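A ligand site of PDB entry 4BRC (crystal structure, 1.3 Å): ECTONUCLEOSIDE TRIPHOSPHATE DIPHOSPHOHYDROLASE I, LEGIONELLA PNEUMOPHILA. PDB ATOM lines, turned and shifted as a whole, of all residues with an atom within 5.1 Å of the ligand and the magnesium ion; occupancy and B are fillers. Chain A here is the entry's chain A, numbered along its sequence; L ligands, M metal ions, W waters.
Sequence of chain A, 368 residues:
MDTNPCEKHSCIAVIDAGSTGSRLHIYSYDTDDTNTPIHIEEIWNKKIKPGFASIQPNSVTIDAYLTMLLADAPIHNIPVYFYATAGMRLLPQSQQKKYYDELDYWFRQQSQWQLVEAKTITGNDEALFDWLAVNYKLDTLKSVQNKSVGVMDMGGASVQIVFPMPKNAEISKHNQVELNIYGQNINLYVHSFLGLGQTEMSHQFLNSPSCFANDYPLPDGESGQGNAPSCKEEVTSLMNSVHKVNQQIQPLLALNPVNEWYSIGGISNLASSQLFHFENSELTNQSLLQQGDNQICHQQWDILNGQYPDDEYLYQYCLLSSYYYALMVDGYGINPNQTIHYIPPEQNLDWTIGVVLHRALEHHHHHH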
ATOM      1  N   ASP A  16     -31.956 -13.549  -1.758  1.00  0.00           N
ATOM      2  CA  ASP A  16     -31.005 -12.985  -2.726  1.00  0.00           C
ATOM      3  C   ASP A  16     -31.057 -13.922  -3.948  1.00  0.00           C
ATOM      4  O   ASP A  16     -30.404 -14.965  -3.885  1.00  0.00           O
ATOM      5  CB  ASP A  16     -29.612 -12.925  -2.081  1.00  0.00           C
ATOM      6  CG  ASP A  16     -28.522 -12.591  -3.036  1.00  0.00           C
ATOM      7  OD1 ASP A  16     -28.750 -12.225  -4.201  1.00  0.00           O
ATOM      8  OD2 ASP A  16     -27.306 -12.710  -2.605  1.00  0.00           O
ATOM      9  N   ALA A  17     -31.830 -13.548  -4.969  1.00  0.00           N
ATOM     10  CA  ALA A  17     -31.833 -14.370  -6.181  1.00  0.00           C
ATOM     11  C   ALA A  17     -30.746 -13.902  -7.110  1.00  0.00           C
ATOM     12  O   ALA A  17     -30.975 -13.066  -7.996  1.00  0.00           O
ATOM     13  CB  ALA A  17     -33.200 -14.377  -6.810  1.00  0.00           C
ATOM     14  N   GLY A  18     -29.510 -14.279  -6.745  1.00  0.00           N
ATOM     15  CA  GLY A  18     -28.336 -13.766  -7.380  1.00  0.00           C
ATOM     16  C   GLY A  18     -27.970 -14.518  -8.684  1.00  0.00           C
ATOM     17  O   GLY A  18     -28.590 -15.522  -9.072  1.00  0.00           O
ATOM     18  N   SER A  19     -26.944 -14.025  -9.365  1.00  0.00           N
ATOM     19  CA  SER A  19     -26.703 -14.543 -10.720  1.00  0.00           C
ATOM     20  C   SER A  19     -26.156 -15.988 -10.679  1.00  0.00           C
ATOM     21  O   SER A  19     -26.414 -16.741 -11.665  1.00  0.00           O
ATOM     22  CB  SER A  19     -25.744 -13.616 -11.513  1.00  0.00           C
ATOM     23  OG  SER A  19     -24.378 -13.791 -11.077  1.00  0.00           O
ATOM     24  N   THR A  20     -25.425 -16.405  -9.636  1.00  0.00           N
ATOM     25  CA  THR A  20     -24.878 -17.786  -9.598  1.00  0.00           C
ATOM     26  C   THR A  20     -25.652 -18.667  -8.624  1.00  0.00           C
ATOM     27  O   THR A  20     -25.356 -19.893  -8.563  1.00  0.00           O
ATOM     28  CB  THR A  20     -23.391 -17.837  -9.242  1.00  0.00           C
ATOM     29  OG1 THR A  20     -23.162 -17.390  -7.895  1.00  0.00           O
ATOM     30  CG2 THR A  20     -22.548 -17.023 -10.231  1.00  0.00           C
ATOM     31  N   GLY A  21     -26.650 -18.133  -7.909  1.00  0.00           N
ATOM     32  CA  GLY A  21     -27.357 -18.934  -6.901  1.00  0.00           C
ATOM     33  C   GLY A  21     -28.357 -18.101  -6.162  1.00  0.00           C
ATOM     34  O   GLY A  21     -28.296 -16.876  -6.242  1.00  0.00           O
ATOM     35  N   ARG A  23     -30.034 -17.407  -2.280  1.00  0.00           N
ATOM     36  CA  ARG A  23     -29.775 -17.551  -0.810  1.00  0.00           C
ATOM     37  C   ARG A  23     -31.002 -17.070  -0.034  1.00  0.00           C
ATOM     38  O   ARG A  23     -31.334 -15.876  -0.112  1.00  0.00           O
ATOM     39  CB  ARG A  23     -28.546 -16.798  -0.411  1.00  0.00           C
ATOM     40  CG  ARG A  23     -27.288 -17.121  -1.221  1.00  0.00           C
ATOM     41  CD  ARG A  23     -27.117 -16.109  -2.336  1.00  0.00           C
ATOM     42  NE  ARG A  23     -26.180 -16.670  -3.344  1.00  0.00           N
ATOM     43  CZ  ARG A  23     -25.671 -15.924  -4.313  1.00  0.00           C
ATOM     44  NH1 ARG A  23     -25.932 -14.584  -4.369  1.00  0.00           N
ATOM     45  NH2 ARG A  23     -24.838 -16.446  -5.162  1.00  0.00           N
ATOM     46  N   THR A  85     -31.345 -10.020  -8.930  1.00  0.00           N
ATOM     47  CA  THR A  85     -30.343  -9.046  -9.210  1.00  0.00           C
ATOM     48  C   THR A  85     -29.884  -9.069 -10.726  1.00  0.00           C
ATOM     49  O   THR A  85     -30.717  -9.270 -11.633  1.00  0.00           O
ATOM     50  CB  THR A  85     -29.169  -9.155  -8.214  1.00  0.00           C
ATOM     51  OG1 THR A  85     -28.654 -10.463  -8.276  1.00  0.00           O
ATOM     52  CG2 THR A  85     -29.660  -8.868  -6.764  1.00  0.00           C
ATOM     53  N   ALA A  86     -28.580  -8.929 -11.015  1.00  0.00           N
ATOM     54  CA  ALA A  86     -28.150  -8.681 -12.349  1.00  0.00           C
ATOM     55  C   ALA A  86     -28.371  -9.841 -13.273  1.00  0.00           C
ATOM     56  O   ALA A  86     -28.504  -9.578 -14.513  1.00  0.00           O
ATOM     57  CB  ALA A  86     -26.701  -8.247 -12.400  1.00  0.00           C
ATOM     58  N   GLY A  87     -28.371 -11.071 -12.851  1.00  0.00           N
ATOM     59  CA  GLY A  87     -28.705 -12.176 -13.777  1.00  0.00           C
ATOM     60  C   GLY A  87     -30.057 -11.990 -14.475  1.00  0.00           C
ATOM     61  O   GLY A  87     -30.221 -12.214 -15.686  1.00  0.00           O
ATOM     62  N   GLU A 126     -29.673  -2.435  -5.231  1.00  0.00           N
ATOM     63  CA  GLU A 126     -28.743  -3.444  -4.784  1.00  0.00           C
ATOM     64  C   GLU A 126     -27.511  -2.782  -4.084  1.00  0.00           C
ATOM     65  O   GLU A 126     -27.071  -3.239  -3.002  1.00  0.00           O
ATOM     66  CB  GLU A 126     -28.313  -4.344  -5.986  1.00  0.00           C
ATOM     67  CG  GLU A 126     -27.464  -5.559  -5.657  1.00  0.00           C
ATOM     68  CD  GLU A 126     -27.179  -6.355  -6.932  1.00  0.00           C
ATOM     69  OE1 GLU A 126     -27.628  -5.907  -8.008  1.00  0.00           O
ATOM     70  OE2 GLU A 126     -26.459  -7.374  -6.853  1.00  0.00           O
ATOM     71  N   ASP A 153     -19.334  -4.632  -3.903  1.00  0.00           N
ATOM     72  CA  ASP A 153     -19.892  -5.991  -3.935  1.00  0.00           C
ATOM     73  C   ASP A 153     -19.460  -6.563  -5.333  1.00  0.00           C
ATOM     74  O   ASP A 153     -19.830  -6.040  -6.381  1.00  0.00           O
ATOM     75  CB  ASP A 153     -21.433  -5.922  -3.794  1.00  0.00           C
ATOM     76  CG  ASP A 153     -22.106  -7.275  -3.867  1.00  0.00           C
ATOM     77  OD1 ASP A 153     -21.434  -8.313  -4.193  1.00  0.00           O
ATOM     78  OD2 ASP A 153     -23.346  -7.283  -3.571  1.00  0.00           O
ATOM     79  N   MET A 154     -18.657  -7.600  -5.225  1.00  0.00           N
ATOM     80  CA  MET A 154     -18.058  -8.263  -6.348  1.00  0.00           C
ATOM     81  C   MET A 154     -18.966  -9.438  -6.765  1.00  0.00           C
ATOM     82  O   MET A 154     -18.706 -10.586  -6.333  1.00  0.00           O
ATOM     83  CB  MET A 154     -16.693  -8.750  -5.863  1.00  0.00           C
ATOM     84  CG  MET A 154     -15.742  -7.618  -5.446  1.00  0.00           C
ATOM     85  SD  MET A 154     -15.656  -6.268  -6.692  1.00  0.00           S
ATOM     86  CE  MET A 154     -14.244  -5.293  -6.072  1.00  0.00           C
ATOM     87  N   GLY A 155     -20.002  -9.205  -7.566  1.00  0.00           N
ATOM     88  CA  GLY A 155     -20.965 -10.216  -7.973  1.00  0.00           C
ATOM     89  C   GLY A 155     -20.509 -10.891  -9.278  1.00  0.00           C
ATOM     90  O   GLY A 155     -19.454 -10.630  -9.837  1.00  0.00           O
ATOM     91  N   GLY A 156     -21.372 -11.785  -9.710  1.00  0.00           N
ATOM     92  CA  GLY A 156     -21.202 -12.588 -10.920  1.00  0.00           C
ATOM     93  C   GLY A 156     -21.698 -11.935 -12.182  1.00  0.00           C
ATOM     94  O   GLY A 156     -21.071 -12.129 -13.282  1.00  0.00           O
ATOM     95  N   ALA A 157     -22.737 -11.102 -12.122  1.00  0.00           N
ATOM     96  CA  ALA A 157     -23.242 -10.407 -13.274  1.00  0.00           C
ATOM     97  C   ALA A 157     -23.083  -8.928 -13.257  1.00  0.00           C
ATOM     98  O   ALA A 157     -22.936  -8.306 -14.276  1.00  0.00           O
ATOM     99  CB  ALA A 157     -24.680 -10.835 -13.636  1.00  0.00           C
ATOM    100  N   SER A 158     -23.020  -8.347 -12.062  1.00  0.00           N
ATOM    101  CA  SER A 158     -22.688  -6.900 -11.910  1.00  0.00           C
ATOM    102  C   SER A 158     -21.744  -6.765 -10.691  1.00  0.00           C
ATOM    103  O   SER A 158     -21.633  -7.679  -9.890  1.00  0.00           O
ATOM    104  CB  SER A 158     -23.936  -5.993 -11.724  1.00  0.00           C
ATOM    105  OG  SER A 158     -24.603  -6.313 -10.506  1.00  0.00           O
ATOM    106  N   GLN A 198     -18.107 -11.190 -12.399  1.00  0.00           N
ATOM    107  CA  GLN A 198     -17.112 -12.252 -12.685  1.00  0.00           C
ATOM    108  C   GLN A 198     -17.457 -13.050 -13.868  1.00  0.00           C
ATOM    109  O   GLN A 198     -16.600 -13.347 -14.715  1.00  0.00           O
ATOM    110  CB  GLN A 198     -17.115 -13.365 -11.616  1.00  0.00           C
ATOM    111  CG  GLN A 198     -16.641 -12.970 -10.315  1.00  0.00           C
ATOM    112  CD  GLN A 198     -16.120 -14.083  -9.441  1.00  0.00           C
ATOM    113  OE1 GLN A 198     -16.209 -15.223  -9.779  1.00  0.00           O
ATOM    114  NE2 GLN A 198     -15.508 -13.728  -8.329  1.00  0.00           N
ATOM    115  N   THR A 199     -18.669 -13.551 -13.878  1.00  0.00           N
ATOM    116  CA  THR A 199     -19.075 -14.563 -14.885  1.00  0.00           C
ATOM    117  C   THR A 199     -19.104 -13.911 -16.233  1.00  0.00           C
ATOM    118  O   THR A 199     -18.502 -14.395 -17.226  1.00  0.00           O
ATOM    119  CB  THR A 199     -20.540 -15.050 -14.696  1.00  0.00           C
ATOM    120  OG1 THR A 199     -20.590 -15.554 -13.391  1.00  0.00           O
ATOM    121  CG2 THR A 199     -20.910 -16.117 -15.760  1.00  0.00           C
ATOM    122  N   GLY A 265     -18.865 -10.419  -1.733  1.00  0.00           N
ATOM    123  CA  GLY A 265     -18.960 -11.136  -3.020  1.00  0.00           C
ATOM    124  C   GLY A 265     -17.770 -12.011  -3.180  1.00  0.00           C
ATOM    125  O   GLY A 265     -17.103 -12.463  -2.197  1.00  0.00           O
ATOM    126  N   GLY A 266     -17.438 -12.276  -4.461  1.00  0.00           N
ATOM    127  CA  GLY A 266     -16.479 -13.374  -4.722  1.00  0.00           C
ATOM    128  C   GLY A 266     -15.088 -13.157  -4.187  1.00  0.00           C
ATOM    129  O   GLY A 266     -14.381 -14.099  -3.878  1.00  0.00           O
ATOM    130  N   ILE A 267     -14.704 -11.848  -4.000  1.00  0.00           N
ATOM    131  CA  ILE A 267     -13.344 -11.575  -3.524  1.00  0.00           C
ATOM    132  C   ILE A 267     -13.170 -12.151  -2.103  1.00  0.00           C
ATOM    133  O   ILE A 267     -12.086 -12.587  -1.736  1.00  0.00           O
ATOM    134  CB  ILE A 267     -13.058 -10.061  -3.531  1.00  0.00           C
ATOM    135  CG1 ILE A 267     -11.578  -9.807  -3.259  1.00  0.00           C
ATOM    136  CG2 ILE A 267     -14.062  -9.243  -2.677  1.00  0.00           C
ATOM    137  CD1 ILE A 267     -11.190  -8.405  -3.638  1.00  0.00           C
ATOM    138  N   ASN A 269     -14.395 -14.946  -0.973  1.00  0.00           N
ATOM    139  CA  ASN A 269     -14.163 -16.398  -1.144  1.00  0.00           C
ATOM    140  C   ASN A 269     -12.770 -16.674  -1.685  1.00  0.00           C
ATOM    141  O   ASN A 269     -12.055 -17.561  -1.196  1.00  0.00           O
ATOM    142  CB  ASN A 269     -15.209 -17.033  -2.062  1.00  0.00           C
ATOM    143  CG  ASN A 269     -16.592 -16.798  -1.534  1.00  0.00           C
ATOM    144  OD1 ASN A 269     -17.210 -15.738  -1.774  1.00  0.00           O
ATOM    145  ND2 ASN A 269     -17.076 -17.756  -0.795  1.00  0.00           N
ATOM    146  N   LEU A 270     -12.320 -15.871  -2.658  1.00  0.00           N
ATOM    147  CA  LEU A 270     -10.948 -15.995  -3.156  1.00  0.00           C
ATOM    148  C   LEU A 270      -9.951 -15.751  -2.056  1.00  0.00           C
ATOM    149  O   LEU A 270      -8.970 -16.520  -1.905  1.00  0.00           O
ATOM    150  CB  LEU A 270     -10.798 -15.050  -4.394  1.00  0.00           C
ATOM    151  CG  LEU A 270      -9.390 -15.042  -4.970  1.00  0.00           C
ATOM    152  CD1 LEU A 270      -9.358 -14.744  -6.477  1.00  0.00           C
ATOM    153  CD2 LEU A 270      -8.402 -14.112  -4.221  1.00  0.00           C
ATOM    154  N   ASP A 311     -10.821 -27.244  -5.000  1.00  0.00           N
ATOM    155  CA  ASP A 311     -11.356 -25.887  -5.100  1.00  0.00           C
ATOM    156  C   ASP A 311     -11.766 -25.661  -6.541  1.00  0.00           C
ATOM    157  O   ASP A 311     -10.903 -25.488  -7.426  1.00  0.00           O
ATOM    158  CB  ASP A 311     -10.287 -24.846  -4.662  1.00  0.00           C
ATOM    159  CG  ASP A 311     -10.810 -23.428  -4.675  1.00  0.00           C
ATOM    160  OD1 ASP A 311     -11.820 -23.131  -5.385  1.00  0.00           O
ATOM    161  OD2 ASP A 311     -10.241 -22.554  -3.947  1.00  0.00           O
ATOM    162  N   TYR A 313     -12.821 -23.205  -8.095  1.00  0.00           N
ATOM    163  CA  TYR A 313     -12.429 -21.904  -8.688  1.00  0.00           C
ATOM    164  C   TYR A 313     -10.928 -21.799  -8.984  1.00  0.00           C
ATOM    165  O   TYR A 313     -10.496 -20.787  -9.564  1.00  0.00           O
ATOM    166  CB  TYR A 313     -12.836 -20.718  -7.787  1.00  0.00           C
ATOM    167  CG  TYR A 313     -14.284 -20.446  -7.781  1.00  0.00           C
ATOM    168  CD1 TYR A 313     -15.152 -21.174  -6.974  1.00  0.00           C
ATOM    169  CD2 TYR A 313     -14.813 -19.498  -8.678  1.00  0.00           C
ATOM    170  CE1 TYR A 313     -16.524 -20.909  -7.027  1.00  0.00           C
ATOM    171  CE2 TYR A 313     -16.165 -19.229  -8.744  1.00  0.00           C
ATOM    172  CZ  TYR A 313     -17.025 -19.921  -7.908  1.00  0.00           C
ATOM    173  OH  TYR A 313     -18.354 -19.659  -8.032  1.00  0.00           O
ATOM    174  N   TYR A 317      -8.221 -18.492 -10.776  1.00  0.00           N
ATOM    175  CA  TYR A 317      -7.678 -17.507  -9.819  1.00  0.00           C
ATOM    176  C   TYR A 317      -6.630 -16.601 -10.379  1.00  0.00           C
ATOM    177  O   TYR A 317      -6.443 -15.496  -9.827  1.00  0.00           O
ATOM    178  CB  TYR A 317      -7.160 -18.268  -8.615  1.00  0.00           C
ATOM    179  CG  TYR A 317      -8.168 -18.759  -7.563  1.00  0.00           C
ATOM    180  CD1 TYR A 317      -9.401 -18.158  -7.376  1.00  0.00           C
ATOM    181  CD2 TYR A 317      -7.835 -19.837  -6.808  1.00  0.00           C
ATOM    182  CE1 TYR A 317     -10.294 -18.592  -6.383  1.00  0.00           C
ATOM    183  CE2 TYR A 317      -8.678 -20.282  -5.744  1.00  0.00           C
ATOM    184  CZ  TYR A 317      -9.910 -19.655  -5.628  1.00  0.00           C
ATOM    185  OH  TYR A 317     -10.822 -20.055  -4.658  1.00  0.00           O
ATOM    186  N   LEU A 320      -9.029 -14.025 -11.886  1.00  0.00           N
ATOM    187  CA  LEU A 320      -9.865 -13.259 -10.934  1.00  0.00           C
ATOM    188  C   LEU A 320      -8.973 -12.327 -10.112  1.00  0.00           C
ATOM    189  O   LEU A 320      -9.397 -11.174  -9.875  1.00  0.00           O
ATOM    190  CB  LEU A 320     -10.646 -14.161  -9.997  1.00  0.00           C
ATOM    191  CG  LEU A 320     -11.774 -14.949 -10.727  1.00  0.00           C
ATOM    192  CD1 LEU A 320     -12.438 -15.914  -9.734  1.00  0.00           C
ATOM    193  CD2 LEU A 320     -12.829 -13.997 -11.365  1.00  0.00           C
ATOM    194  N   TYR A 324      -9.792  -8.341 -10.190  1.00  0.00           N
ATOM    195  CA  TYR A 324     -10.069  -7.496  -8.992  1.00  0.00           C
ATOM    196  C   TYR A 324      -9.136  -6.294  -8.970  1.00  0.00           C
ATOM    197  O   TYR A 324      -9.566  -5.183  -8.643  1.00  0.00           O
ATOM    198  CB  TYR A 324      -9.938  -8.283  -7.644  1.00  0.00           C
ATOM    199  CG  TYR A 324     -10.914  -9.434  -7.451  1.00  0.00           C
ATOM    200  CD1 TYR A 324     -12.269  -9.319  -7.815  1.00  0.00           C
ATOM    201  CD2 TYR A 324     -10.510 -10.618  -6.885  1.00  0.00           C
ATOM    202  CE1 TYR A 324     -13.160 -10.353  -7.684  1.00  0.00           C
ATOM    203  CE2 TYR A 324     -11.417 -11.665  -6.686  1.00  0.00           C
ATOM    204  CZ  TYR A 324     -12.731 -11.548  -7.100  1.00  0.00           C
ATOM    205  OH  TYR A 324     -13.582 -12.647  -6.972  1.00  0.00           O
ATOM    206  N   TRP A 351     -26.516  -8.440   0.682  1.00  0.00           N
ATOM    207  CA  TRP A 351     -27.293  -7.201   0.736  1.00  0.00           C
ATOM    208  C   TRP A 351     -28.679  -7.380   1.354  1.00  0.00           C
ATOM    209  O   TRP A 351     -29.349  -6.378   1.570  1.00  0.00           O
ATOM    210  CB  TRP A 351     -27.343  -6.578  -0.666  1.00  0.00           C
ATOM    211  CG  TRP A 351     -27.847  -7.547  -1.671  1.00  0.00           C
ATOM    212  CD1 TRP A 351     -27.034  -8.233  -2.590  1.00  0.00           C
ATOM    213  CD2 TRP A 351     -29.180  -7.920  -1.967  1.00  0.00           C
ATOM    214  NE1 TRP A 351     -27.816  -9.071  -3.392  1.00  0.00           N
ATOM    215  CE2 TRP A 351     -29.131  -8.899  -3.060  1.00  0.00           C
ATOM    216  CE3 TRP A 351     -30.431  -7.548  -1.470  1.00  0.00           C
ATOM    217  CZ2 TRP A 351     -30.252  -9.521  -3.565  1.00  0.00           C
ATOM    218  CZ3 TRP A 351     -31.580  -8.121  -2.022  1.00  0.00           C
ATOM    219  CH2 TRP A 351     -31.488  -9.105  -3.047  1.00  0.00           C
HETATM  220  O1  LIG L   1     -24.358 -12.883  -5.960  1.00  0.00           O
HETATM  221  P1  LIG L   1     -23.709 -13.480  -7.218  1.00  0.00           P
HETATM  222  O2  LIG L   1     -24.051 -14.893  -7.477  1.00  0.00           O
HETATM  223  N1  LIG L   1     -24.027 -12.583  -8.611  1.00  0.00           N
HETATM  224  P2  LIG L   1     -24.833 -11.102  -8.603  1.00  0.00           P
HETATM  225  O3  LIG L   1     -24.342 -10.421  -9.843  1.00  0.00           O
HETATM  226  O4  LIG L   1     -26.310 -11.416  -8.720  1.00  0.00           O
HETATM  227  O5  LIG L   1     -24.476 -10.361  -7.293  1.00  0.00           O
HETATM  228  O6  LIG L   1     -22.092 -13.312  -7.078  1.00  0.00           O
HETATM  229  C1  LIG L   1     -21.302 -14.081  -6.226  1.00  0.00           C
HETATM  230  C2  LIG L   1     -19.983 -14.243  -6.930  1.00  0.00           C
HETATM  231  C3  LIG L   1     -20.085 -15.144  -8.156  1.00  0.00           C
HETATM  232  O7  LIG L   1     -19.368 -14.508  -9.254  1.00  0.00           O
HETATM  233  C4  LIG L   1     -19.326 -16.420  -7.771  1.00  0.00           C
HETATM  234  O8  LIG L   1     -18.814 -17.108  -8.939  1.00  0.00           O
HETATM  235  C5  LIG L   1     -18.267 -15.796  -6.882  1.00  0.00           C
HETATM  236  O9  LIG L   1     -19.040 -14.918  -6.075  1.00  0.00           O
HETATM  237  N2  LIG L   1     -17.484 -16.777  -6.100  1.00  0.00           N
HETATM  238  C6  LIG L   1     -16.133 -16.802  -6.037  1.00  0.00           C
HETATM  239  C7  LIG L   1     -15.706 -17.923  -5.273  1.00  0.00           C
HETATM  240  N3  LIG L   1     -16.910 -18.502  -4.817  1.00  0.00           N
HETATM  241  C8  LIG L   1     -17.948 -17.813  -5.330  1.00  0.00           C
HETATM  242  N4  LIG L   1     -15.265 -15.952  -6.626  1.00  0.00           N
HETATM  243  C9  LIG L   1     -13.970 -16.227  -6.367  1.00  0.00           C
HETATM  244  N5  LIG L   1     -13.442 -17.269  -5.697  1.00  0.00           N
HETATM  245  C10 LIG L   1     -14.314 -18.162  -5.124  1.00  0.00           C
HETATM  246  N6  LIG L   1     -13.745 -19.166  -4.392  1.00  0.00           N
HETATM  247 MG    MG M   1     -24.704 -10.935  -5.398  1.00  0.00          MG
HETATM  248  O   HOH W   1     -19.831 -19.420 -11.200  1.00  0.00           O
HETATM  249  O   HOH W   2     -22.720 -10.672  -4.834  1.00  0.00           O
HETATM  250  O   HOH W   3     -26.817 -11.129  -5.668  1.00  0.00           O
HETATM  251  O   HOH W   4     -25.065 -11.493  -3.399  1.00  0.00           O
HETATM  252  O   HOH W   5     -19.518 -14.816  -3.196  1.00  0.00           O
HETATM  253  O   HOH W   6     -17.304 -20.701  -3.249  1.00  0.00           O
HETATM  254  O   HOH W   7     -21.967 -15.421  -3.102  1.00  0.00           O
HETATM  255  O   HOH W   8     -25.040  -8.908  -4.929  1.00  0.00           O
HETATM  256  O   HOH W   9     -23.307  -7.890  -7.485  1.00  0.00           O
HETATM  257  O   HOH W  10     -13.686 -22.012  -3.654  1.00  0.00           O
HETATM  258  O   HOH W  11     -26.113  -8.279  -9.350  1.00  0.00           O
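The backbone NH of Thr 85 sits at hydrogen-bond distance from the backbone carbonyl oxygen of Ala 17 (3.2 Å). OG1 of Thr 20 lies within hydrogen-bond range of NH2 of Arg 23, 3.3 Å away. The side-chain hydroxyl (OH) of Tyr 324 sits at hydrogen-bond distance from the side-chain amide nitrogen (NE2) of Gln 198 (2.6 Å). The backbone NH (N) of Thr 199 is in hydrogen-bond range of the backbone carbonyl oxygen (O) of Gly 156. The side-chain carboxylate (OD2) of Asp 311 lies within hydrogen-bond range of the side-chain hydroxyl (OH) of Tyr 317 (2.7 Å). The backbone NH (N) of Gly 266 is in hydrogen-bond range of the backbone carbonyl oxygen (O) of Met 154, 2.8 Å away. O of Gly 265 sits close to OD1 of Asn 269 (3.3 Å). OH of Tyr 324 is in hydrogen-bond range of N of Ile 267 (3.3 Å).
The magnesium ion is bound by O5 of the ligand, O1 of the ligand, water W2, water W4, water W8 and water W3.
An oxygen (O4) of the ligand is in hydrogen-bond range of the side-chain hydroxyl of Thr 85, 2.6 Å away. N of Thr 20 lies within hydrogen-bond range of O2 of the ligand (3.0 Å). O2 of the ligand is in hydrogen-bond range of OG1 of Thr 20, 2.7 Å away. The side-chain hydroxyl (OH) of Tyr 313 is in hydrogen-bond range of an oxygen (O8) of the ligand, 2.7 Å away. The backbone NH of Ser 19 sits at hydrogen-bond distance from an oxygen (O4) of the ligand. OG of Ser 19 sits at hydrogen-bond distance from N1 of the ligand, at 2.8 Å. N4 of the ligand sits at hydrogen-bond distance from NE2 of Gln 198 (2.8 Å). O2 of the ligand is in salt-bridge range of NH2 of Arg 23 (2.9 Å). An oxygen (O3) of the ligand lies within hydrogen-bond range of the backbone NH (N) of Ala 157. An oxygen (O6) of the ligand lies within hydrogen-bond range of the backbone NH (N) of Gly 156 (3.1 Å). A nitrogen (N6) of the ligand sits at hydrogen-bond distance from the side-chain hydroxyl of Tyr 317. N of Gly 266 lies close to O9 of the ligand (3.5 Å). The backbone NH (N) of Ser 158 sits at hydrogen-bond distance from an oxygen (O3) of the ligand, at 3.3 Å.
CA of Gly 18 touches O4 of the ligand (3.4 Å). Glu 126 touches the ligand. Met 154 touches the ligand. CA of Gly 155 touches O6 of the ligand (3.4 Å). CB of Asn 269 touches C7 of the ligand, 3.4 Å away. Leu 270 touches the ligand. CD1 of Leu 320 touches C9 of the ligand (3.7 Å). OH of Tyr 324 touches C9 of the ligand, 3.7 Å away. Hydrophobic or aromatic side chains within 4 Å of the ligand: Ala 157, Leu 270, Tyr 313, Tyr 317 and Leu 320. Of the 30 residues printed, 19 come within 4 Å of the ligand. The nearest printed residue that does not touch the ligand is Ala 86 (4.1 Å).
Arg 23 touches the magnesium ion (NH1 to MG, 3.99 Å). Of the 30 residues printed, 1 comes within 4 Å of the magnesium ion.
Water W4 bridges the side-chain carboxylate (OD2) of Asp 16 (2.7 Å) and the guanidinium group (NH1) of Arg 23 (3.4 Å). Water W3 lies within hydrogen-bond range of OD1 of Asp 16, O4 of the ligand, NE1 of Trp 351 and OG1 of Thr 85. Water W9 bridges O of Ser 158 (2.9 Å) and OE2 of Glu 126 (3.3 Å). Water W11 lies within hydrogen-bond range of OE2 of Glu 126 (2.7 Å), OG of Ser 158 (2.7 Å), O3 of the ligand (2.8 Å) and N of Ala 86 (3.0 Å). Water W5 bridges OD1 of Asn 269 and O9 of the ligand. Water W10 lies within hydrogen-bond range of the side-chain carboxylate of Asp 311 (2.8 Å) and a nitrogen (N6) of the ligand (2.9 Å).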
